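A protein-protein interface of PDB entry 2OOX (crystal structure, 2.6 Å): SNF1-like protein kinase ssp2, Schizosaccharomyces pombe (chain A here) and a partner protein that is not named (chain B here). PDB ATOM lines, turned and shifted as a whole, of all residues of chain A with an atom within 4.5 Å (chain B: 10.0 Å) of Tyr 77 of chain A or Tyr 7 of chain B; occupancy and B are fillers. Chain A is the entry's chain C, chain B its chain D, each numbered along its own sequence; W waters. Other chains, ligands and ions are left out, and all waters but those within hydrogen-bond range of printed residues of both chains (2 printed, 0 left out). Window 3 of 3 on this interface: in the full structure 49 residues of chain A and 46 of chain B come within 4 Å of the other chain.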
ATOM      1  N   GLN A  40       9.338  -7.228   0.780  1.00  0.00           N
ATOM      2  CA  GLN A  40       9.381  -7.042  -0.662  1.00  0.00           C
ATOM      3  C   GLN A  40       8.270  -7.919  -1.263  1.00  0.00           C
ATOM      4  O   GLN A  40       7.936  -8.962  -0.724  1.00  0.00           O
ATOM      5  CB  GLN A  40      10.794  -7.357  -1.200  1.00  0.00           C
ATOM      6  CG  GLN A  40      11.933  -6.911  -0.241  1.00  0.00           C
ATOM      7  CD  GLN A  40      13.359  -7.000  -0.833  1.00  0.00           C
ATOM      8  OE1 GLN A  40      14.119  -7.946  -0.547  1.00  0.00           O
ATOM      9  NE2 GLN A  40      13.731  -6.002  -1.642  1.00  0.00           N
ATOM     10  N   PHE A  41       7.669  -7.491  -2.361  1.00  0.00           N
ATOM     11  CA  PHE A  41       6.407  -8.094  -2.787  1.00  0.00           C
ATOM     12  C   PHE A  41       6.162  -8.010  -4.286  1.00  0.00           C
ATOM     13  O   PHE A  41       6.737  -7.167  -4.969  1.00  0.00           O
ATOM     14  CB  PHE A  41       5.256  -7.408  -2.052  1.00  0.00           C
ATOM     15  CG  PHE A  41       5.481  -5.946  -1.820  1.00  0.00           C
ATOM     16  CD1 PHE A  41       5.317  -5.028  -2.856  1.00  0.00           C
ATOM     17  CD2 PHE A  41       5.882  -5.483  -0.571  1.00  0.00           C
ATOM     18  CE1 PHE A  41       5.532  -3.665  -2.644  1.00  0.00           C
ATOM     19  CE2 PHE A  41       6.108  -4.124  -0.347  1.00  0.00           C
ATOM     20  CZ  PHE A  41       5.934  -3.208  -1.374  1.00  0.00           C
ATOM     21  N   THR A  42       5.298  -8.883  -4.784  1.00  0.00           N
ATOM     22  CA  THR A  42       4.866  -8.811  -6.165  1.00  0.00           C
ATOM     23  C   THR A  42       3.766  -7.769  -6.346  1.00  0.00           C
ATOM     24  O   THR A  42       3.006  -7.476  -5.417  1.00  0.00           O
ATOM     25  CB  THR A  42       4.320 -10.152  -6.695  1.00  0.00           C
ATOM     26  OG1 THR A  42       3.007 -10.374  -6.167  1.00  0.00           O
ATOM     27  CG2 THR A  42       5.247 -11.319  -6.369  1.00  0.00           C
ATOM     28  N   LYS A  59       2.088 -12.668  -2.337  1.00  0.00           N
ATOM     29  CA  LYS A  59       3.358 -13.365  -2.118  1.00  0.00           C
ATOM     30  C   LYS A  59       4.567 -12.423  -2.009  1.00  0.00           C
ATOM     31  O   LYS A  59       5.003 -11.790  -2.970  1.00  0.00           O
ATOM     32  CB  LYS A  59       3.559 -14.578  -3.055  1.00  0.00           C
ATOM     33  CG  LYS A  59       4.101 -14.361  -4.456  1.00  0.00           C
ATOM     34  CD  LYS A  59       3.565 -15.445  -5.415  1.00  0.00           C
ATOM     35  CE  LYS A  59       4.204 -16.831  -5.214  1.00  0.00           C
ATOM     36  NZ  LYS A  59       5.133 -17.251  -6.322  1.00  0.00           N
ATOM     37  N   SER A  60       5.066 -12.336  -0.782  1.00  0.00           N
ATOM     38  CA  SER A  60       6.067 -11.378  -0.384  1.00  0.00           C
ATOM     39  C   SER A  60       7.304 -12.150  -0.031  1.00  0.00           C
ATOM     40  O   SER A  60       7.301 -13.378  -0.039  1.00  0.00           O
ATOM     41  CB  SER A  60       5.576 -10.635   0.862  1.00  0.00           C
ATOM     42  OG  SER A  60       5.084 -11.551   1.848  1.00  0.00           O
ATOM     43  N   ARG A  61       8.347 -11.411   0.311  1.00  0.00           N
ATOM     44  CA  ARG A  61       9.630 -11.958   0.696  1.00  0.00           C
ATOM     45  C   ARG A  61      10.188 -11.088   1.846  1.00  0.00           C
ATOM     46  O   ARG A  61      10.171  -9.851   1.758  1.00  0.00           O
ATOM     47  CB  ARG A  61      10.555 -11.998  -0.538  1.00  0.00           C
ATOM     48  CG  ARG A  61      12.017 -12.275  -0.266  1.00  0.00           C
ATOM     49  CD  ARG A  61      12.714 -12.849  -1.486  1.00  0.00           C
ATOM     50  NE  ARG A  61      13.413 -11.912  -2.377  1.00  0.00           N
ATOM     51  CZ  ARG A  61      13.439 -10.585  -2.261  1.00  0.00           C
ATOM     52  NH1 ARG A  61      12.801  -9.970  -1.268  1.00  0.00           N
ATOM     53  NH2 ARG A  61      14.118  -9.869  -3.153  1.00  0.00           N
ATOM     54  N   TYR A  75      15.784 -15.608   3.685  1.00  0.00           N
ATOM     55  CA  TYR A  75      14.499 -14.994   3.421  1.00  0.00           C
ATOM     56  C   TYR A  75      13.349 -15.898   3.771  1.00  0.00           C
ATOM     57  O   TYR A  75      13.429 -17.101   3.607  1.00  0.00           O
ATOM     58  CB  TYR A  75      14.389 -14.564   1.941  1.00  0.00           C
ATOM     59  CG  TYR A  75      15.406 -13.515   1.518  1.00  0.00           C
ATOM     60  CD1 TYR A  75      15.720 -12.441   2.363  1.00  0.00           C
ATOM     61  CD2 TYR A  75      16.038 -13.588   0.270  1.00  0.00           C
ATOM     62  CE1 TYR A  75      16.656 -11.478   1.999  1.00  0.00           C
ATOM     63  CE2 TYR A  75      16.971 -12.620  -0.120  1.00  0.00           C
ATOM     64  CZ  TYR A  75      17.280 -11.569   0.758  1.00  0.00           C
ATOM     65  OH  TYR A  75      18.209 -10.611   0.402  1.00  0.00           O
ATOM     66  N   ALA A  76      12.274 -15.299   4.249  1.00  0.00           N
ATOM     67  CA  ALA A  76      11.026 -16.008   4.426  1.00  0.00           C
ATOM     68  C   ALA A  76      10.094 -15.605   3.304  1.00  0.00           C
ATOM     69  O   ALA A  76      10.031 -14.426   2.947  1.00  0.00           O
ATOM     70  CB  ALA A  76      10.417 -15.664   5.759  1.00  0.00           C
ATOM     71  N   TYR A  77       9.368 -16.592   2.772  1.00  0.00           N
ATOM     72  CA  TYR A  77       8.473 -16.436   1.624  1.00  0.00           C
ATOM     73  C   TYR A  77       7.028 -16.587   2.078  1.00  0.00           C
ATOM     74  O   TYR A  77       6.572 -17.679   2.412  1.00  0.00           O
ATOM     75  CB  TYR A  77       8.818 -17.463   0.546  1.00  0.00           C
ATOM     76  CG  TYR A  77      10.179 -17.231  -0.080  1.00  0.00           C
ATOM     77  CD1 TYR A  77      10.308 -16.480  -1.254  1.00  0.00           C
ATOM     78  CD2 TYR A  77      11.340 -17.747   0.499  1.00  0.00           C
ATOM     79  CE1 TYR A  77      11.541 -16.259  -1.834  1.00  0.00           C
ATOM     80  CE2 TYR A  77      12.577 -17.525  -0.067  1.00  0.00           C
ATOM     81  CZ  TYR A  77      12.675 -16.775  -1.235  1.00  0.00           C
ATOM     82  OH  TYR A  77      13.915 -16.532  -1.809  1.00  0.00           O
ATOM     83  N   ILE A  78       6.300 -15.481   2.101  1.00  0.00           N
ATOM     84  CA  ILE A  78       4.954 -15.457   2.652  1.00  0.00           C
ATOM     85  C   ILE A  78       3.940 -14.994   1.603  1.00  0.00           C
ATOM     86  O   ILE A  78       4.064 -13.910   1.029  1.00  0.00           O
ATOM     87  CB  ILE A  78       4.933 -14.559   3.913  1.00  0.00           C
ATOM     88  CG1 ILE A  78       5.787 -15.214   5.024  1.00  0.00           C
ATOM     89  CG2 ILE A  78       3.494 -14.289   4.371  1.00  0.00           C
ATOM     90  CD1 ILE A  78       6.144 -14.344   6.246  1.00  0.00           C
ATOM     91  N   GLU A  79       2.930 -15.810   1.358  1.00  0.00           N
ATOM     92  CA  GLU A  79       1.938 -15.515   0.310  1.00  0.00           C
ATOM     93  C   GLU A  79       0.593 -15.096   0.907  1.00  0.00           C
ATOM     94  O   GLU A  79       0.006 -15.833   1.692  1.00  0.00           O
ATOM     95  CB  GLU A  79       1.772 -16.739  -0.613  1.00  0.00           C
ATOM     96  CG  GLU A  79       0.795 -16.585  -1.786  1.00  0.00           C
ATOM     97  CD  GLU A  79       0.774 -17.832  -2.710  1.00  0.00           C
ATOM     98  OE1 GLU A  79       1.872 -18.393  -2.970  1.00  0.00           O
ATOM     99  OE2 GLU A  79      -0.333 -18.245  -3.168  1.00  0.00           O
ATOM    100  N   LYS A  95      -0.072 -17.370   4.304  1.00  0.00           N
ATOM    101  CA  LYS A  95       0.452 -18.732   4.212  1.00  0.00           C
ATOM    102  C   LYS A  95       1.965 -18.737   4.096  1.00  0.00           C
ATOM    103  O   LYS A  95       2.563 -17.945   3.358  1.00  0.00           O
ATOM    104  CB  LYS A  95      -0.189 -19.475   3.038  1.00  0.00           C
ATOM    105  CG  LYS A  95       0.679 -20.563   2.377  1.00  0.00           C
ATOM    106  CD  LYS A  95       0.063 -21.071   1.049  1.00  0.00           C
ATOM    107  CE  LYS A  95       0.861 -22.252   0.458  1.00  0.00           C
ATOM    108  NZ  LYS A  95       0.946 -23.484   1.343  1.00  0.00           N
ATOM    109  N   SER A  96       2.585 -19.627   4.854  1.00  0.00           N
ATOM    110  CA  SER A  96       4.019 -19.805   4.781  1.00  0.00           C
ATOM    111  C   SER A  96       4.353 -20.712   3.618  1.00  0.00           C
ATOM    112  O   SER A  96       3.800 -21.796   3.492  1.00  0.00           O
ATOM    113  CB  SER A  96       4.551 -20.420   6.076  1.00  0.00           C
ATOM    114  OG  SER A  96       5.948 -20.637   5.986  1.00  0.00           O
ATOM    115  N   ASN A  97       5.236 -20.267   2.746  1.00  0.00           N
ATOM    116  CA  ASN A  97       5.919 -21.248   1.925  1.00  0.00           C
ATOM    117  C   ASN A  97       7.436 -21.264   2.073  1.00  0.00           C
ATOM    118  O   ASN A  97       8.173 -21.235   1.080  1.00  0.00           O
ATOM    119  CB  ASN A  97       5.375 -21.414   0.472  1.00  0.00           C
ATOM    120  CG  ASN A  97       4.963 -20.127  -0.172  1.00  0.00           C
ATOM    121  OD1 ASN A  97       3.914 -20.064  -0.830  1.00  0.00           O
ATOM    122  ND2 ASN A  97       5.790 -19.091  -0.017  1.00  0.00           N
ATOM    123  N   GLY A  98       7.875 -21.297   3.338  1.00  0.00           N
ATOM    124  CA  GLY A  98       9.218 -21.698   3.701  1.00  0.00           C
ATOM    125  C   GLY A  98      10.264 -20.624   3.754  1.00  0.00           C
ATOM    126  O   GLY A  98       9.953 -19.450   3.682  1.00  0.00           O
ATOM    127  N   LYS A 100      14.712 -19.736   2.860  1.00  0.00           N
ATOM    128  CA  LYS A 100      15.899 -20.023   2.041  1.00  0.00           C
ATOM    129  C   LYS A 100      17.028 -19.033   2.366  1.00  0.00           C
ATOM    130  O   LYS A 100      16.814 -17.824   2.319  1.00  0.00           O
ATOM    131  CB  LYS A 100      15.517 -19.953   0.550  1.00  0.00           C
ATOM    132  CG  LYS A 100      16.500 -20.596  -0.469  1.00  0.00           C
ATOM    133  CD  LYS A 100      17.784 -19.774  -0.684  1.00  0.00           C
ATOM    134  CE  LYS A 100      17.481 -18.354  -1.128  1.00  0.00           C
ATOM    135  NZ  LYS A 100      18.601 -17.430  -0.856  1.00  0.00           N
ATOM    136  N   ASP A 111      11.290 -21.984  -2.731  1.00  0.00           N
ATOM    137  CA  ASP A 111      11.717 -21.326  -1.479  1.00  0.00           C
ATOM    138  C   ASP A 111      12.391 -22.239  -0.438  1.00  0.00           C
ATOM    139  O   ASP A 111      12.349 -21.950   0.763  1.00  0.00           O
ATOM    140  CB  ASP A 111      10.572 -20.541  -0.854  1.00  0.00           C
ATOM    141  N   SER B   4       6.062 -14.783  -9.236  1.00  0.00           N
ATOM    142  CA  SER B   4       7.224 -14.578  -8.314  1.00  0.00           C
ATOM    143  C   SER B   4       8.231 -13.525  -8.820  1.00  0.00           C
ATOM    144  O   SER B   4       7.862 -12.635  -9.590  1.00  0.00           O
ATOM    145  CB  SER B   4       7.933 -15.907  -8.059  1.00  0.00           C
ATOM    146  OG  SER B   4       7.326 -16.624  -7.002  1.00  0.00           O
ATOM    147  N   GLU B   5       9.487 -13.641  -8.368  1.00  0.00           N
ATOM    148  CA  GLU B   5      10.641 -12.797  -8.780  1.00  0.00           C
ATOM    149  C   GLU B   5      10.292 -11.429  -9.397  1.00  0.00           C
ATOM    150  O   GLU B   5      10.134 -11.289 -10.612  1.00  0.00           O
ATOM    151  CB  GLU B   5      11.580 -13.588  -9.693  1.00  0.00           C
ATOM    152  CG  GLU B   5      10.900 -14.228 -10.900  1.00  0.00           C
ATOM    153  CD  GLU B   5      11.864 -15.054 -11.709  1.00  0.00           C
ATOM    154  OE1 GLU B   5      12.754 -15.691 -11.083  1.00  0.00           O
ATOM    155  OE2 GLU B   5      11.732 -15.066 -12.962  1.00  0.00           O
ATOM    156  N   GLN B   6      10.203 -10.418  -8.546  1.00  0.00           N
ATOM    157  CA  GLN B   6       9.480  -9.205  -8.874  1.00  0.00           C
ATOM    158  C   GLN B   6       9.533  -8.339  -7.649  1.00  0.00           C
ATOM    159  O   GLN B   6       9.392  -7.119  -7.708  1.00  0.00           O
ATOM    160  CB  GLN B   6       8.021  -9.570  -9.160  1.00  0.00           C
ATOM    161  CG  GLN B   6       7.030  -8.420  -9.245  1.00  0.00           C
ATOM    162  CD  GLN B   6       5.668  -8.871  -9.732  1.00  0.00           C
ATOM    163  OE1 GLN B   6       4.762  -8.063  -9.877  1.00  0.00           O
ATOM    164  NE2 GLN B   6       5.518 -10.166  -9.990  1.00  0.00           N
ATOM    165  N   TYR B   7       9.720  -9.008  -6.527  1.00  0.00           N
ATOM    166  CA  TYR B   7       9.877  -8.376  -5.240  1.00  0.00           C
ATOM    167  C   TYR B   7      10.439  -6.963  -5.368  1.00  0.00           C
ATOM    168  O   TYR B   7      11.502  -6.755  -5.958  1.00  0.00           O
ATOM    169  CB  TYR B   7      10.762  -9.261  -4.377  1.00  0.00           C
ATOM    170  CG  TYR B   7      10.291 -10.700  -4.302  1.00  0.00           C
ATOM    171  CD1 TYR B   7      11.113 -11.745  -4.709  1.00  0.00           C
ATOM    172  CD2 TYR B   7       9.023 -11.011  -3.812  1.00  0.00           C
ATOM    173  CE1 TYR B   7      10.694 -13.057  -4.621  1.00  0.00           C
ATOM    174  CE2 TYR B   7       8.595 -12.333  -3.717  1.00  0.00           C
ATOM    175  CZ  TYR B   7       9.437 -13.345  -4.124  1.00  0.00           C
ATOM    176  OH  TYR B   7       9.013 -14.643  -4.030  1.00  0.00           O
ATOM    177  N   SER B   8       9.701  -5.994  -4.827  1.00  0.00           N
ATOM    178  CA  SER B   8       9.989  -4.587  -5.104  1.00  0.00           C
ATOM    179  C   SER B   8       9.513  -3.593  -4.051  1.00  0.00           C
ATOM    180  O   SER B   8       9.193  -3.946  -2.917  1.00  0.00           O
ATOM    181  CB  SER B   8       9.387  -4.193  -6.468  1.00  0.00           C
ATOM    182  OG  SER B   8       8.050  -4.659  -6.601  1.00  0.00           O
ATOM    183  N   THR B   9       9.539  -2.333  -4.470  1.00  0.00           N
ATOM    184  CA  THR B   9       8.785  -1.237  -3.885  1.00  0.00           C
ATOM    185  C   THR B   9       8.380  -0.290  -5.065  1.00  0.00           C
ATOM    186  O   THR B   9       8.947  -0.393  -6.160  1.00  0.00           O
ATOM    187  CB  THR B   9       9.614  -0.528  -2.767  1.00  0.00           C
ATOM    188  OG1 THR B   9       8.719   0.053  -1.813  1.00  0.00           O
ATOM    189  CG2 THR B   9      10.583   0.556  -3.324  1.00  0.00           C
ATOM    190  N   GLU B  10       7.388   0.582  -4.895  1.00  0.00           N
ATOM    191  CA  GLU B  10       6.532   0.609  -3.726  1.00  0.00           C
ATOM    192  C   GLU B  10       5.131   0.178  -4.129  1.00  0.00           C
ATOM    193  O   GLU B  10       4.955  -0.599  -5.073  1.00  0.00           O
ATOM    194  CB  GLU B  10       6.561   1.997  -3.032  1.00  0.00           C
ATOM    195  CG  GLU B  10       5.819   3.178  -3.714  1.00  0.00           C
ATOM    196  CD  GLU B  10       5.408   4.278  -2.715  1.00  0.00           C
ATOM    197  OE1 GLU B  10       4.274   4.798  -2.843  1.00  0.00           O
ATOM    198  OE2 GLU B  10       6.203   4.612  -1.800  1.00  0.00           O
ATOM    199  N   ASN B  62       0.540 -24.689   7.445  1.00  0.00           N
ATOM    200  CA  ASN B  62       1.069 -23.331   7.491  1.00  0.00           C
ATOM    201  C   ASN B  62       0.242 -22.157   7.009  1.00  0.00           C
ATOM    202  O   ASN B  62       0.779 -21.209   6.493  1.00  0.00           O
ATOM    203  CB  ASN B  62       2.498 -23.288   7.019  1.00  0.00           C
ATOM    204  CG  ASN B  62       3.459 -23.693   8.131  1.00  0.00           C
ATOM    205  OD1 ASN B  62       4.080 -24.766   8.056  1.00  0.00           O
ATOM    206  ND2 ASN B  62       3.550 -22.858   9.205  1.00  0.00           N
HETATM  207  O   HOH W   1       6.441 -15.550  -2.055  1.00  0.00           O
HETATM  208  O   HOH W   2       6.202 -22.490   8.173  1.00  0.00           O
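Of the 17 printed residues of chain A, 9 touch a printed residue of chain B.
Printed residues of chain A that touch a printed residue of chain B: Gln 40, Phe 41, Thr 42, Lys 59, Ser 60, Arg 61, Tyr 77, Lys 95 and Ser 96.
Hydrophobic or aromatic side chains of chain A that line the printed part of chain B: Phe 41 and Tyr 77.
Printed residues of chain B that touch a printed residue of chain A: Ser 4, Gln 6, Tyr 7, Ser 8, Glu 10 and Asn 62.
Hydrophobic or aromatic side chains of chain B within 4 Å of the printed part of chain A: Tyr 7.
Along chain B the printed residues that touch a printed residue of chain A span positions 4 to 62.
Water W2 lies within hydrogen-bond range of ND2 of Asn 62 of chain B (2.9 Å) and OG of Ser 96 of chain A (2.9 Å).
Water W1 lies within hydrogen-bond range of the backbone carbonyl oxygen (O) of Ser 60 of chain A (3.1 Å) and the side-chain hydroxyl (OH) of Tyr 7 of chain B (3.4 Å).
Of the printed residues of chain B, Thr 42 of chain A touches Gln 6 (3.5 Å).
Ser 60 of chain A touches just one residue of chain B: Tyr 7.
Arg 61 of chain A touches just one residue of chain B: Tyr 7 (3.3 Å).
No residue of chain B comes within 4 Å of Ala 76 of chain A.
Of chain B, only Tyr 7 (3.6 Å) comes within 4 Å of Tyr 77 of chain A.
No residue of chain B comes within 4 Å of Ile 78 of chain A.
Glu 79 of chain A touches none of the printed residues of chain B.
No residue of chain B comes within 4 Å of Asn 97 of chain A.
No residue of chain B comes within 4 Å of Gly 98 of chain A.
No residue of chain B comes within 4 Å of Lys 100 of chain A.
Printed residues of chain A within 4 Å of Gln 6 of chain B: Phe 41 (3.8 Å) and Thr 42 (3.5 Å).
Of chain A, only Gln 40, Phe 41, Lys 59, Ser 60, Arg 61 and Tyr 77 come within 4 Å of Tyr 7 of chain B.
Thr 9 of chain B touches none of the printed residues of chain A.
The nearest residue of chain B that does not touch Tyr 77 of chain A is Ser 4 of chain B (6.5 Å).
The nearest printed residue of chain A that does not touch Glu 10 of chain B is Thr 42 of chain A (7.2 Å).
The backbone NH (N) of Thr 42 of chain A is in hydrogen-bond range of the backbone carbonyl oxygen (O) of Lys 59 of chain A (3.4 Å).
O of Ile 78 of chain A is in hydrogen-bond range of N of Ser 60 of chain A (2.6 Å).
The backbone carbonyl oxygen of Tyr 77 of chain A is in hydrogen-bond range of the side-chain amide nitrogen of Asn 97 of chain A.
O of Gly 98 of chain A sits at hydrogen-bond distance from N of Tyr 77 of chain A.
The side-chain hydroxyl of Ser 96 of chain A sits at hydrogen-bond distance from the backbone NH of Gly 98 of chain A (3.3 Å).
The side-chain hydroxyl of Ser 8 of chain B is in hydrogen-bond range of the backbone carbonyl oxygen of Gln 6 of chain B (3.0 Å).
CB of Gln 40 of chain A touches CB of Tyr 7 of chain B, at 3.7 Å.
O of Ser 8 of chain B touches CA of Gln 40 of chain A, 3.8 Å away.
Phe 41 of chain A touches Gln 6 of chain B (O to O, 3.8 Å).
Phe 41 of chain A touches Tyr 7 of chain B (O to CA, 3.4 Å).
O of Glu 10 of chain B touches CE1 of Phe 41 of chain A, 3.95 Å away.
CB of Thr 42 of chain A touches NE2 of Gln 6 of chain B, 3.5 Å away.
Lys 59 of chain A touches Tyr 7 of chain B.
Ser 60 of chain A touches Tyr 7 of chain B.
CD1 of Tyr 77 of chain A touches OH of Tyr 7 of chain B, at 3.6 Å.
Lys 95 of chain A touches Asn 62 of chain B.
O of Phe 41 of chain A is in hydrogen-bond range of N of Ser 8 of chain B.
N of Ser 96 of chain A lies within hydrogen-bond range of O of Asn 62 of chain B (2.9 Å).
NZ of Lys 59 of chain A sits close to OG of Ser 4 of chain B (2.4 Å).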
